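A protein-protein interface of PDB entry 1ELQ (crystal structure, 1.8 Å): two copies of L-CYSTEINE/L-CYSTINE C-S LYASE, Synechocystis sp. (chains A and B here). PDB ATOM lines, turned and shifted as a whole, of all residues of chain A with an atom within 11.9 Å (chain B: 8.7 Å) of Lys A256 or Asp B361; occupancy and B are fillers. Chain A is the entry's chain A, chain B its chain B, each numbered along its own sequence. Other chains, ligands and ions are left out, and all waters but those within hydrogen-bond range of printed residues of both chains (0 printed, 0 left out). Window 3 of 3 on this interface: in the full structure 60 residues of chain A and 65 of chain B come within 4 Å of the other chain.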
ATOM      1  N   ILE A 251      -0.900  39.825   5.587  1.00  0.00           N
ATOM      2  CA  ILE A 251      -0.502  40.311   4.278  1.00  0.00           C
ATOM      3  C   ILE A 251      -1.456  40.296   3.094  1.00  0.00           C
ATOM      4  O   ILE A 251      -2.526  39.707   3.141  1.00  0.00           O
ATOM      5  CB  ILE A 251       0.735  39.507   3.866  1.00  0.00           C
ATOM      6  CG1 ILE A 251       0.368  38.017   3.778  1.00  0.00           C
ATOM      7  CG2 ILE A 251       1.818  39.668   4.923  1.00  0.00           C
ATOM      8  CD1 ILE A 251       1.518  37.075   3.393  1.00  0.00           C
ATOM      9  N   THR A 252      -1.030  40.971   2.021  1.00  0.00           N
ATOM     10  CA  THR A 252      -1.763  40.982   0.756  1.00  0.00           C
ATOM     11  C   THR A 252      -0.924  40.027  -0.063  1.00  0.00           C
ATOM     12  O   THR A 252       0.261  39.849   0.219  1.00  0.00           O
ATOM     13  CB  THR A 252      -1.792  42.369   0.058  1.00  0.00           C
ATOM     14  OG1 THR A 252      -0.466  42.901  -0.018  1.00  0.00           O
ATOM     15  CG2 THR A 252      -2.679  43.311   0.813  1.00  0.00           C
ATOM     16  N   TYR A 253      -1.512  39.438  -1.097  1.00  0.00           N
ATOM     17  CA  TYR A 253      -0.789  38.441  -1.881  1.00  0.00           C
ATOM     18  C   TYR A 253      -0.558  38.741  -3.356  1.00  0.00           C
ATOM     19  O   TYR A 253      -1.346  39.411  -3.990  1.00  0.00           O
ATOM     20  CB  TYR A 253      -1.513  37.087  -1.763  1.00  0.00           C
ATOM     21  CG  TYR A 253      -1.522  36.463  -0.372  1.00  0.00           C
ATOM     22  CD1 TYR A 253      -2.408  36.890   0.612  1.00  0.00           C
ATOM     23  CD2 TYR A 253      -0.627  35.441  -0.056  1.00  0.00           C
ATOM     24  CE1 TYR A 253      -2.405  36.306   1.897  1.00  0.00           C
ATOM     25  CE2 TYR A 253      -0.603  34.864   1.197  1.00  0.00           C
ATOM     26  CZ  TYR A 253      -1.491  35.293   2.170  1.00  0.00           C
ATOM     27  OH  TYR A 253      -1.450  34.683   3.393  1.00  0.00           O
ATOM     28  N   GLY A 254       0.538  38.203  -3.883  1.00  0.00           N
ATOM     29  CA  GLY A 254       0.889  38.387  -5.278  1.00  0.00           C
ATOM     30  C   GLY A 254       0.292  37.281  -6.126  1.00  0.00           C
ATOM     31  O   GLY A 254      -0.297  36.327  -5.608  1.00  0.00           O
ATOM     32  N   ALA A 255       0.449  37.414  -7.439  1.00  0.00           N
ATOM     33  CA  ALA A 255      -0.079  36.438  -8.382  1.00  0.00           C
ATOM     34  C   ALA A 255       0.411  35.022  -8.102  1.00  0.00           C
ATOM     35  O   ALA A 255      -0.290  34.057  -8.407  1.00  0.00           O
ATOM     36  CB  ALA A 255       0.282  36.846  -9.806  1.00  0.00           C
ATOM     37  N   LYS A 256       1.596  34.888  -7.515  1.00  0.00           N
ATOM     38  CA  LYS A 256       2.117  33.556  -7.232  1.00  0.00           C
ATOM     39  C   LYS A 256       1.951  33.118  -5.779  1.00  0.00           C
ATOM     40  O   LYS A 256       2.608  32.174  -5.321  1.00  0.00           O
ATOM     41  CB  LYS A 256       3.589  33.469  -7.631  1.00  0.00           C
ATOM     42  CG  LYS A 256       3.824  33.492  -9.139  1.00  0.00           C
ATOM     43  CD  LYS A 256       5.262  33.099  -9.485  1.00  0.00           C
ATOM     44  CE  LYS A 256       5.550  31.631  -9.158  1.00  0.00           C
ATOM     45  NZ  LYS A 256       6.893  31.170  -9.643  1.00  0.00           N
ATOM     46  N   GLY A 257       1.077  33.809  -5.059  1.00  0.00           N
ATOM     47  CA  GLY A 257       0.836  33.483  -3.660  1.00  0.00           C
ATOM     48  C   GLY A 257       1.874  34.066  -2.708  1.00  0.00           C
ATOM     49  O   GLY A 257       1.865  33.752  -1.524  1.00  0.00           O
ATOM     50  N   GLU A 258       2.760  34.917  -3.225  1.00  0.00           N
ATOM     51  CA  GLU A 258       3.809  35.538  -2.419  1.00  0.00           C
ATOM     52  C   GLU A 258       3.310  36.801  -1.705  1.00  0.00           C
ATOM     53  O   GLU A 258       2.401  37.465  -2.180  1.00  0.00           O
ATOM     54  CB  GLU A 258       5.014  35.908  -3.306  1.00  0.00           C
ATOM     55  CG  GLU A 258       4.809  37.147  -4.164  1.00  0.00           C
ATOM     56  CD  GLU A 258       4.001  36.915  -5.439  1.00  0.00           C
ATOM     57  OE1 GLU A 258       3.014  36.147  -5.435  1.00  0.00           O
ATOM     58  OE2 GLU A 258       4.351  37.542  -6.463  1.00  0.00           O
ATOM     59  N   PRO A 259       3.909  37.144  -0.551  1.00  0.00           N
ATOM     60  CA  PRO A 259       3.512  38.336   0.208  1.00  0.00           C
ATOM     61  C   PRO A 259       3.860  39.591  -0.591  1.00  0.00           C
ATOM     62  O   PRO A 259       4.973  39.698  -1.107  1.00  0.00           O
ATOM     63  CB  PRO A 259       4.365  38.248   1.478  1.00  0.00           C
ATOM     64  CG  PRO A 259       4.743  36.768   1.568  1.00  0.00           C
ATOM     65  CD  PRO A 259       4.995  36.421   0.131  1.00  0.00           C
ATOM     66  N   THR A 260       2.931  40.538  -0.678  1.00  0.00           N
ATOM     67  CA  THR A 260       3.178  41.774  -1.421  1.00  0.00           C
ATOM     68  C   THR A 260       2.996  43.037  -0.587  1.00  0.00           C
ATOM     69  O   THR A 260       3.216  44.153  -1.074  1.00  0.00           O
ATOM     70  CB  THR A 260       2.246  41.893  -2.651  1.00  0.00           C
ATOM     71  OG1 THR A 260       0.883  41.711  -2.237  1.00  0.00           O
ATOM     72  CG2 THR A 260       2.613  40.843  -3.695  1.00  0.00           C
ATOM     73  N   GLY A 261       2.588  42.884   0.662  1.00  0.00           N
ATOM     74  CA  GLY A 261       2.416  44.063   1.492  1.00  0.00           C
ATOM     75  C   GLY A 261       1.661  43.718   2.751  1.00  0.00           C
ATOM     76  O   GLY A 261       1.458  42.539   3.014  1.00  0.00           O
ATOM     77  N   ASP B 108      12.798  27.265  -0.973  1.00  0.00           N
ATOM     78  CA  ASP B 108      11.907  28.002  -1.855  1.00  0.00           C
ATOM     79  C   ASP B 108      10.480  27.422  -1.783  1.00  0.00           C
ATOM     80  O   ASP B 108       9.662  27.666  -2.667  1.00  0.00           O
ATOM     81  CB  ASP B 108      12.428  27.960  -3.304  1.00  0.00           C
ATOM     82  CG  ASP B 108      12.501  26.553  -3.872  1.00  0.00           C
ATOM     83  OD1 ASP B 108      12.707  26.429  -5.096  1.00  0.00           O
ATOM     84  OD2 ASP B 108      12.370  25.564  -3.126  1.00  0.00           O
ATOM     85  N   CYS B 109      10.192  26.663  -0.725  1.00  0.00           N
ATOM     86  CA  CYS B 109       8.868  26.054  -0.548  1.00  0.00           C
ATOM     87  C   CYS B 109       8.251  26.367   0.812  1.00  0.00           C
ATOM     88  O   CYS B 109       7.489  25.558   1.338  1.00  0.00           O
ATOM     89  CB  CYS B 109       8.950  24.543  -0.706  1.00  0.00           C
ATOM     90  SG  CYS B 109       9.322  24.046  -2.417  1.00  0.00           S
ATOM     91  N   GLU B 110       8.588  27.527   1.373  1.00  0.00           N
ATOM     92  CA  GLU B 110       8.058  27.917   2.675  1.00  0.00           C
ATOM     93  C   GLU B 110       6.734  28.668   2.532  1.00  0.00           C
ATOM     94  O   GLU B 110       6.414  29.222   1.480  1.00  0.00           O
ATOM     95  CB  GLU B 110       9.083  28.753   3.447  1.00  0.00           C
ATOM     96  CG  GLU B 110      10.335  27.966   3.789  1.00  0.00           C
ATOM     97  CD  GLU B 110      10.034  26.553   4.288  1.00  0.00           C
ATOM     98  OE1 GLU B 110       9.295  26.390   5.278  1.00  0.00           O
ATOM     99  OE2 GLU B 110      10.542  25.585   3.691  1.00  0.00           O
ATOM    100  N   PRO B 112       3.776  31.384   2.838  1.00  0.00           N
ATOM    101  CA  PRO B 112       3.804  32.847   2.715  1.00  0.00           C
ATOM    102  C   PRO B 112       3.860  33.596   4.035  1.00  0.00           C
ATOM    103  O   PRO B 112       4.532  34.631   4.137  1.00  0.00           O
ATOM    104  CB  PRO B 112       2.534  33.177   1.912  1.00  0.00           C
ATOM    105  CG  PRO B 112       1.673  31.962   2.040  1.00  0.00           C
ATOM    106  CD  PRO B 112       2.688  30.815   2.026  1.00  0.00           C
ATOM    107  N   ILE B 115       7.506  33.641   5.433  1.00  0.00           N
ATOM    108  CA  ILE B 115       8.321  34.539   4.621  1.00  0.00           C
ATOM    109  C   ILE B 115       8.081  35.955   5.129  1.00  0.00           C
ATOM    110  O   ILE B 115       9.015  36.723   5.344  1.00  0.00           O
ATOM    111  CB  ILE B 115       7.905  34.441   3.110  1.00  0.00           C
ATOM    112  CG1 ILE B 115       8.377  33.120   2.531  1.00  0.00           C
ATOM    113  CG2 ILE B 115       8.427  35.640   2.323  1.00  0.00           C
ATOM    114  CD1 ILE B 115       7.927  32.896   1.078  1.00  0.00           C
ATOM    115  N   ALA B 135      12.457  22.683  -4.168  1.00  0.00           N
ATOM    116  CA  ALA B 135      11.315  22.151  -4.916  1.00  0.00           C
ATOM    117  C   ALA B 135      11.772  21.141  -5.959  1.00  0.00           C
ATOM    118  O   ALA B 135      11.210  20.046  -6.090  1.00  0.00           O
ATOM    119  CB  ALA B 135      10.537  23.287  -5.585  1.00  0.00           C
ATOM    120  N   LEU B 164       7.016  19.357   2.880  1.00  0.00           N
ATOM    121  CA  LEU B 164       6.629  20.527   2.073  1.00  0.00           C
ATOM    122  C   LEU B 164       5.139  20.592   1.774  1.00  0.00           C
ATOM    123  O   LEU B 164       4.570  19.638   1.268  1.00  0.00           O
ATOM    124  CB  LEU B 164       7.418  20.544   0.745  1.00  0.00           C
ATOM    125  CG  LEU B 164       8.960  20.528   0.805  1.00  0.00           C
ATOM    126  CD1 LEU B 164       9.543  20.859  -0.568  1.00  0.00           C
ATOM    127  CD2 LEU B 164       9.444  21.567   1.816  1.00  0.00           C
ATOM    128  N   TRP B 165       4.523  21.731   2.079  1.00  0.00           N
ATOM    129  CA  TRP B 165       3.080  21.918   1.880  1.00  0.00           C
ATOM    130  C   TRP B 165       2.616  22.004   0.425  1.00  0.00           C
ATOM    131  O   TRP B 165       1.416  21.835   0.139  1.00  0.00           O
ATOM    132  CB  TRP B 165       2.618  23.185   2.625  1.00  0.00           C
ATOM    133  CG  TRP B 165       2.807  24.465   1.867  1.00  0.00           C
ATOM    134  CD1 TRP B 165       3.939  24.894   1.209  1.00  0.00           C
ATOM    135  CD2 TRP B 165       1.854  25.522   1.747  1.00  0.00           C
ATOM    136  NE1 TRP B 165       3.741  26.156   0.693  1.00  0.00           N
ATOM    137  CE2 TRP B 165       2.471  26.564   1.011  1.00  0.00           C
ATOM    138  CE3 TRP B 165       0.534  25.693   2.196  1.00  0.00           C
ATOM    139  CZ2 TRP B 165       1.810  27.768   0.714  1.00  0.00           C
ATOM    140  CZ3 TRP B 165      -0.128  26.900   1.897  1.00  0.00           C
ATOM    141  CH2 TRP B 165       0.521  27.914   1.164  1.00  0.00           C
ATOM    142  N   ASN B 166       3.550  22.304  -0.477  1.00  0.00           N
ATOM    143  CA  ASN B 166       3.234  22.420  -1.889  1.00  0.00           C
ATOM    144  C   ASN B 166       3.527  21.160  -2.724  1.00  0.00           C
ATOM    145  O   ASN B 166       2.670  20.728  -3.517  1.00  0.00           O
ATOM    146  CB  ASN B 166       3.932  23.656  -2.511  1.00  0.00           C
ATOM    147  CG  ASN B 166       5.469  23.659  -2.356  1.00  0.00           C
ATOM    148  OD1 ASN B 166       6.150  24.430  -3.025  1.00  0.00           O
ATOM    149  ND2 ASN B 166       5.997  22.838  -1.482  1.00  0.00           N
ATOM    150  N   THR B 167       4.701  20.555  -2.533  1.00  0.00           N
ATOM    151  CA  THR B 167       5.057  19.371  -3.316  1.00  0.00           C
ATOM    152  C   THR B 167       4.922  18.050  -2.602  1.00  0.00           C
ATOM    153  O   THR B 167       4.887  17.015  -3.254  1.00  0.00           O
ATOM    154  CB  THR B 167       6.509  19.437  -3.838  1.00  0.00           C
ATOM    155  OG1 THR B 167       7.420  19.362  -2.738  1.00  0.00           O
ATOM    156  CG2 THR B 167       6.740  20.706  -4.615  1.00  0.00           C
ATOM    157  N   LEU B 322       3.310  15.312  -9.366  1.00  0.00           N
ATOM    158  CA  LEU B 322       4.602  15.967  -9.300  1.00  0.00           C
ATOM    159  C   LEU B 322       5.679  14.935  -8.950  1.00  0.00           C
ATOM    160  O   LEU B 322       6.789  15.029  -9.439  1.00  0.00           O
ATOM    161  CB  LEU B 322       4.623  17.080  -8.251  1.00  0.00           C
ATOM    162  CG  LEU B 322       3.638  18.227  -8.485  1.00  0.00           C
ATOM    163  CD1 LEU B 322       4.091  19.473  -7.730  1.00  0.00           C
ATOM    164  CD2 LEU B 322       3.549  18.522  -9.968  1.00  0.00           C
ATOM    165  N   SER B 333       0.530  15.779  -4.709  1.00  0.00           N
ATOM    166  CA  SER B 333       0.302  16.908  -5.614  1.00  0.00           C
ATOM    167  C   SER B 333       0.382  16.483  -7.062  1.00  0.00           C
ATOM    168  O   SER B 333       1.165  15.598  -7.426  1.00  0.00           O
ATOM    169  CB  SER B 333       1.296  18.043  -5.355  1.00  0.00           C
ATOM    170  OG  SER B 333       1.034  18.662  -4.109  1.00  0.00           O
ATOM    171  N   THR B 358      -6.157  23.967  -3.967  1.00  0.00           N
ATOM    172  CA  THR B 358      -5.331  24.518  -5.050  1.00  0.00           C
ATOM    173  C   THR B 358      -4.002  25.013  -4.421  1.00  0.00           C
ATOM    174  O   THR B 358      -3.995  25.607  -3.341  1.00  0.00           O
ATOM    175  CB  THR B 358      -6.067  25.706  -5.735  1.00  0.00           C
ATOM    176  OG1 THR B 358      -7.249  25.205  -6.377  1.00  0.00           O
ATOM    177  CG2 THR B 358      -5.224  26.328  -6.787  1.00  0.00           C
ATOM    178  N   ILE B 359      -2.882  24.724  -5.067  1.00  0.00           N
ATOM    179  CA  ILE B 359      -1.562  25.166  -4.607  1.00  0.00           C
ATOM    180  C   ILE B 359      -1.115  26.299  -5.539  1.00  0.00           C
ATOM    181  O   ILE B 359      -1.204  26.158  -6.766  1.00  0.00           O
ATOM    182  CB  ILE B 359      -0.546  24.003  -4.681  1.00  0.00           C
ATOM    183  CG1 ILE B 359      -0.972  22.878  -3.726  1.00  0.00           C
ATOM    184  CG2 ILE B 359       0.837  24.520  -4.360  1.00  0.00           C
ATOM    185  CD1 ILE B 359      -1.010  23.315  -2.254  1.00  0.00           C
ATOM    186  N   ALA B 360      -0.643  27.415  -4.980  1.00  0.00           N
ATOM    187  CA  ALA B 360      -0.253  28.573  -5.807  1.00  0.00           C
ATOM    188  C   ALA B 360       1.063  28.409  -6.555  1.00  0.00           C
ATOM    189  O   ALA B 360       1.186  28.821  -7.720  1.00  0.00           O
ATOM    190  CB  ALA B 360      -0.201  29.841  -4.953  1.00  0.00           C
ATOM    191  N   ASP B 361       2.035  27.796  -5.889  1.00  0.00           N
ATOM    192  CA  ASP B 361       3.338  27.563  -6.479  1.00  0.00           C
ATOM    193  C   ASP B 361       3.935  26.241  -5.980  1.00  0.00           C
ATOM    194  O   ASP B 361       4.162  26.038  -4.779  1.00  0.00           O
ATOM    195  CB  ASP B 361       4.256  28.737  -6.130  1.00  0.00           C
ATOM    196  CG  ASP B 361       5.656  28.591  -6.714  1.00  0.00           C
ATOM    197  OD1 ASP B 361       5.790  28.326  -7.925  1.00  0.00           O
ATOM    198  OD2 ASP B 361       6.624  28.753  -5.941  1.00  0.00           O
ATOM    199  N   PRO B 362       4.130  25.290  -6.888  1.00  0.00           N
ATOM    200  CA  PRO B 362       3.826  25.375  -8.315  1.00  0.00           C
ATOM    201  C   PRO B 362       2.307  25.319  -8.492  1.00  0.00           C
ATOM    202  O   PRO B 362       1.595  24.848  -7.614  1.00  0.00           O
ATOM    203  CB  PRO B 362       4.528  24.148  -8.874  1.00  0.00           C
ATOM    204  CG  PRO B 362       4.387  23.165  -7.772  1.00  0.00           C
ATOM    205  CD  PRO B 362       4.729  23.980  -6.554  1.00  0.00           C
ATOM    206  N   ASP B 363       1.806  25.811  -9.618  1.00  0.00           N
ATOM    207  CA  ASP B 363       0.359  25.792  -9.877  1.00  0.00           C
ATOM    208  C   ASP B 363      -0.108  24.331 -10.015  1.00  0.00           C
ATOM    209  O   ASP B 363       0.114  23.689 -11.035  1.00  0.00           O
ATOM    210  CB  ASP B 363       0.062  26.590 -11.147  1.00  0.00           C
ATOM    211  CG  ASP B 363      -1.371  26.487 -11.571  1.00  0.00           C
ATOM    212  OD1 ASP B 363      -1.670  26.895 -12.709  1.00  0.00           O
ATOM    213  OD2 ASP B 363      -2.198  26.004 -10.784  1.00  0.00           O
ATOM    214  N   CYS B 364      -0.723  23.794  -8.968  1.00  0.00           N
ATOM    215  CA  CYS B 364      -1.168  22.396  -8.972  1.00  0.00           C
ATOM    216  C   CYS B 364      -2.291  22.191  -7.973  1.00  0.00           C
ATOM    217  O   CYS B 364      -2.767  23.147  -7.348  1.00  0.00           O
ATOM    218  CB  CYS B 364       0.003  21.448  -8.619  1.00  0.00           C
ATOM    219  SG  CYS B 364       0.710  21.671  -6.932  1.00  0.00           S
ATOM    220  N   ILE B 365      -2.741  20.945  -7.842  1.00  0.00           N
ATOM    221  CA  ILE B 365      -3.794  20.609  -6.886  1.00  0.00           C
ATOM    222  C   ILE B 365      -3.174  19.641  -5.890  1.00  0.00           C
ATOM    223  O   ILE B 365      -2.317  18.826  -6.262  1.00  0.00           O
ATOM    224  CB  ILE B 365      -4.994  19.953  -7.586  1.00  0.00           C
ATOM    225  CG1 ILE B 365      -5.682  20.999  -8.479  1.00  0.00           C
ATOM    226  CG2 ILE B 365      -5.943  19.366  -6.542  1.00  0.00           C
ATOM    227  CD1 ILE B 365      -6.835  20.478  -9.380  1.00  0.00           C
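NZ of Lys A256 is in salt-bridge range of OD1 of Asp B361 (3.5 Å).
The side-chain hydroxyl (OG1) of Thr A260 lies close to the backbone NH (N) of Tyr A253 (3.5 Å). The side-chain carboxylate (OE1) of Glu A258 sits at hydrogen-bond distance from the backbone NH (N) of Lys A256, at 2.8 Å. The side-chain amide oxygen of Asn B166 sits close to the backbone carbonyl oxygen of Asp B361.
Ile A251 touches Pro B112. Tyr A253 touches Pro B112. O of Lys A256 touches CB of Ala B360 (3.7 Å). O of Gly A257 touches CB of Pro B112, 3.5 Å away. CG of Pro A259 touches O of Pro B112, at 3.3 Å. Pro A259 touches Ile B115.
Of the printed residues of chain B, Tyr A253 touches Pro B112 (3.6 Å). Gly A254 touches none of the printed residues of chain B. Lys A256 touches two residues of chain B. No residue of chain A comes within 4 Å of Cys B109. Of the printed residues of chain A, Pro B112 touches Ile A251 (3.95 Å), Tyr A253 (3.6 Å), Gly A257 (3.5 Å) and Pro A259 (3.3 Å). Of the printed residues of chain A, Ile B115 touches Pro A259. No residue of chain A comes within 4 Å of Asn B166. Asp B361 touches one residue of chain A. Pro B362 touches none of the printed residues of chain A. No residue of chain A comes within 4 Å of Asp B363. No residue of chain A comes within 4 Å of Cys B364. The nearest printed residue of chain B that does not touch Ile A251 is Ile B115 (6.9 Å).
Among the printed residues, 7 pairs touch across the chains. Among the printed residues, Asp or Glu carboxylates within 4 Å of a Lys or Arg side-chain nitrogen of the other chain: Lys A256 with Asp B361 (3.5 Å).
No position is printed for both chains. Of the 7 pairs that touch across the chains among the printed residues, none has its exchanged pair printed and touching as well.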
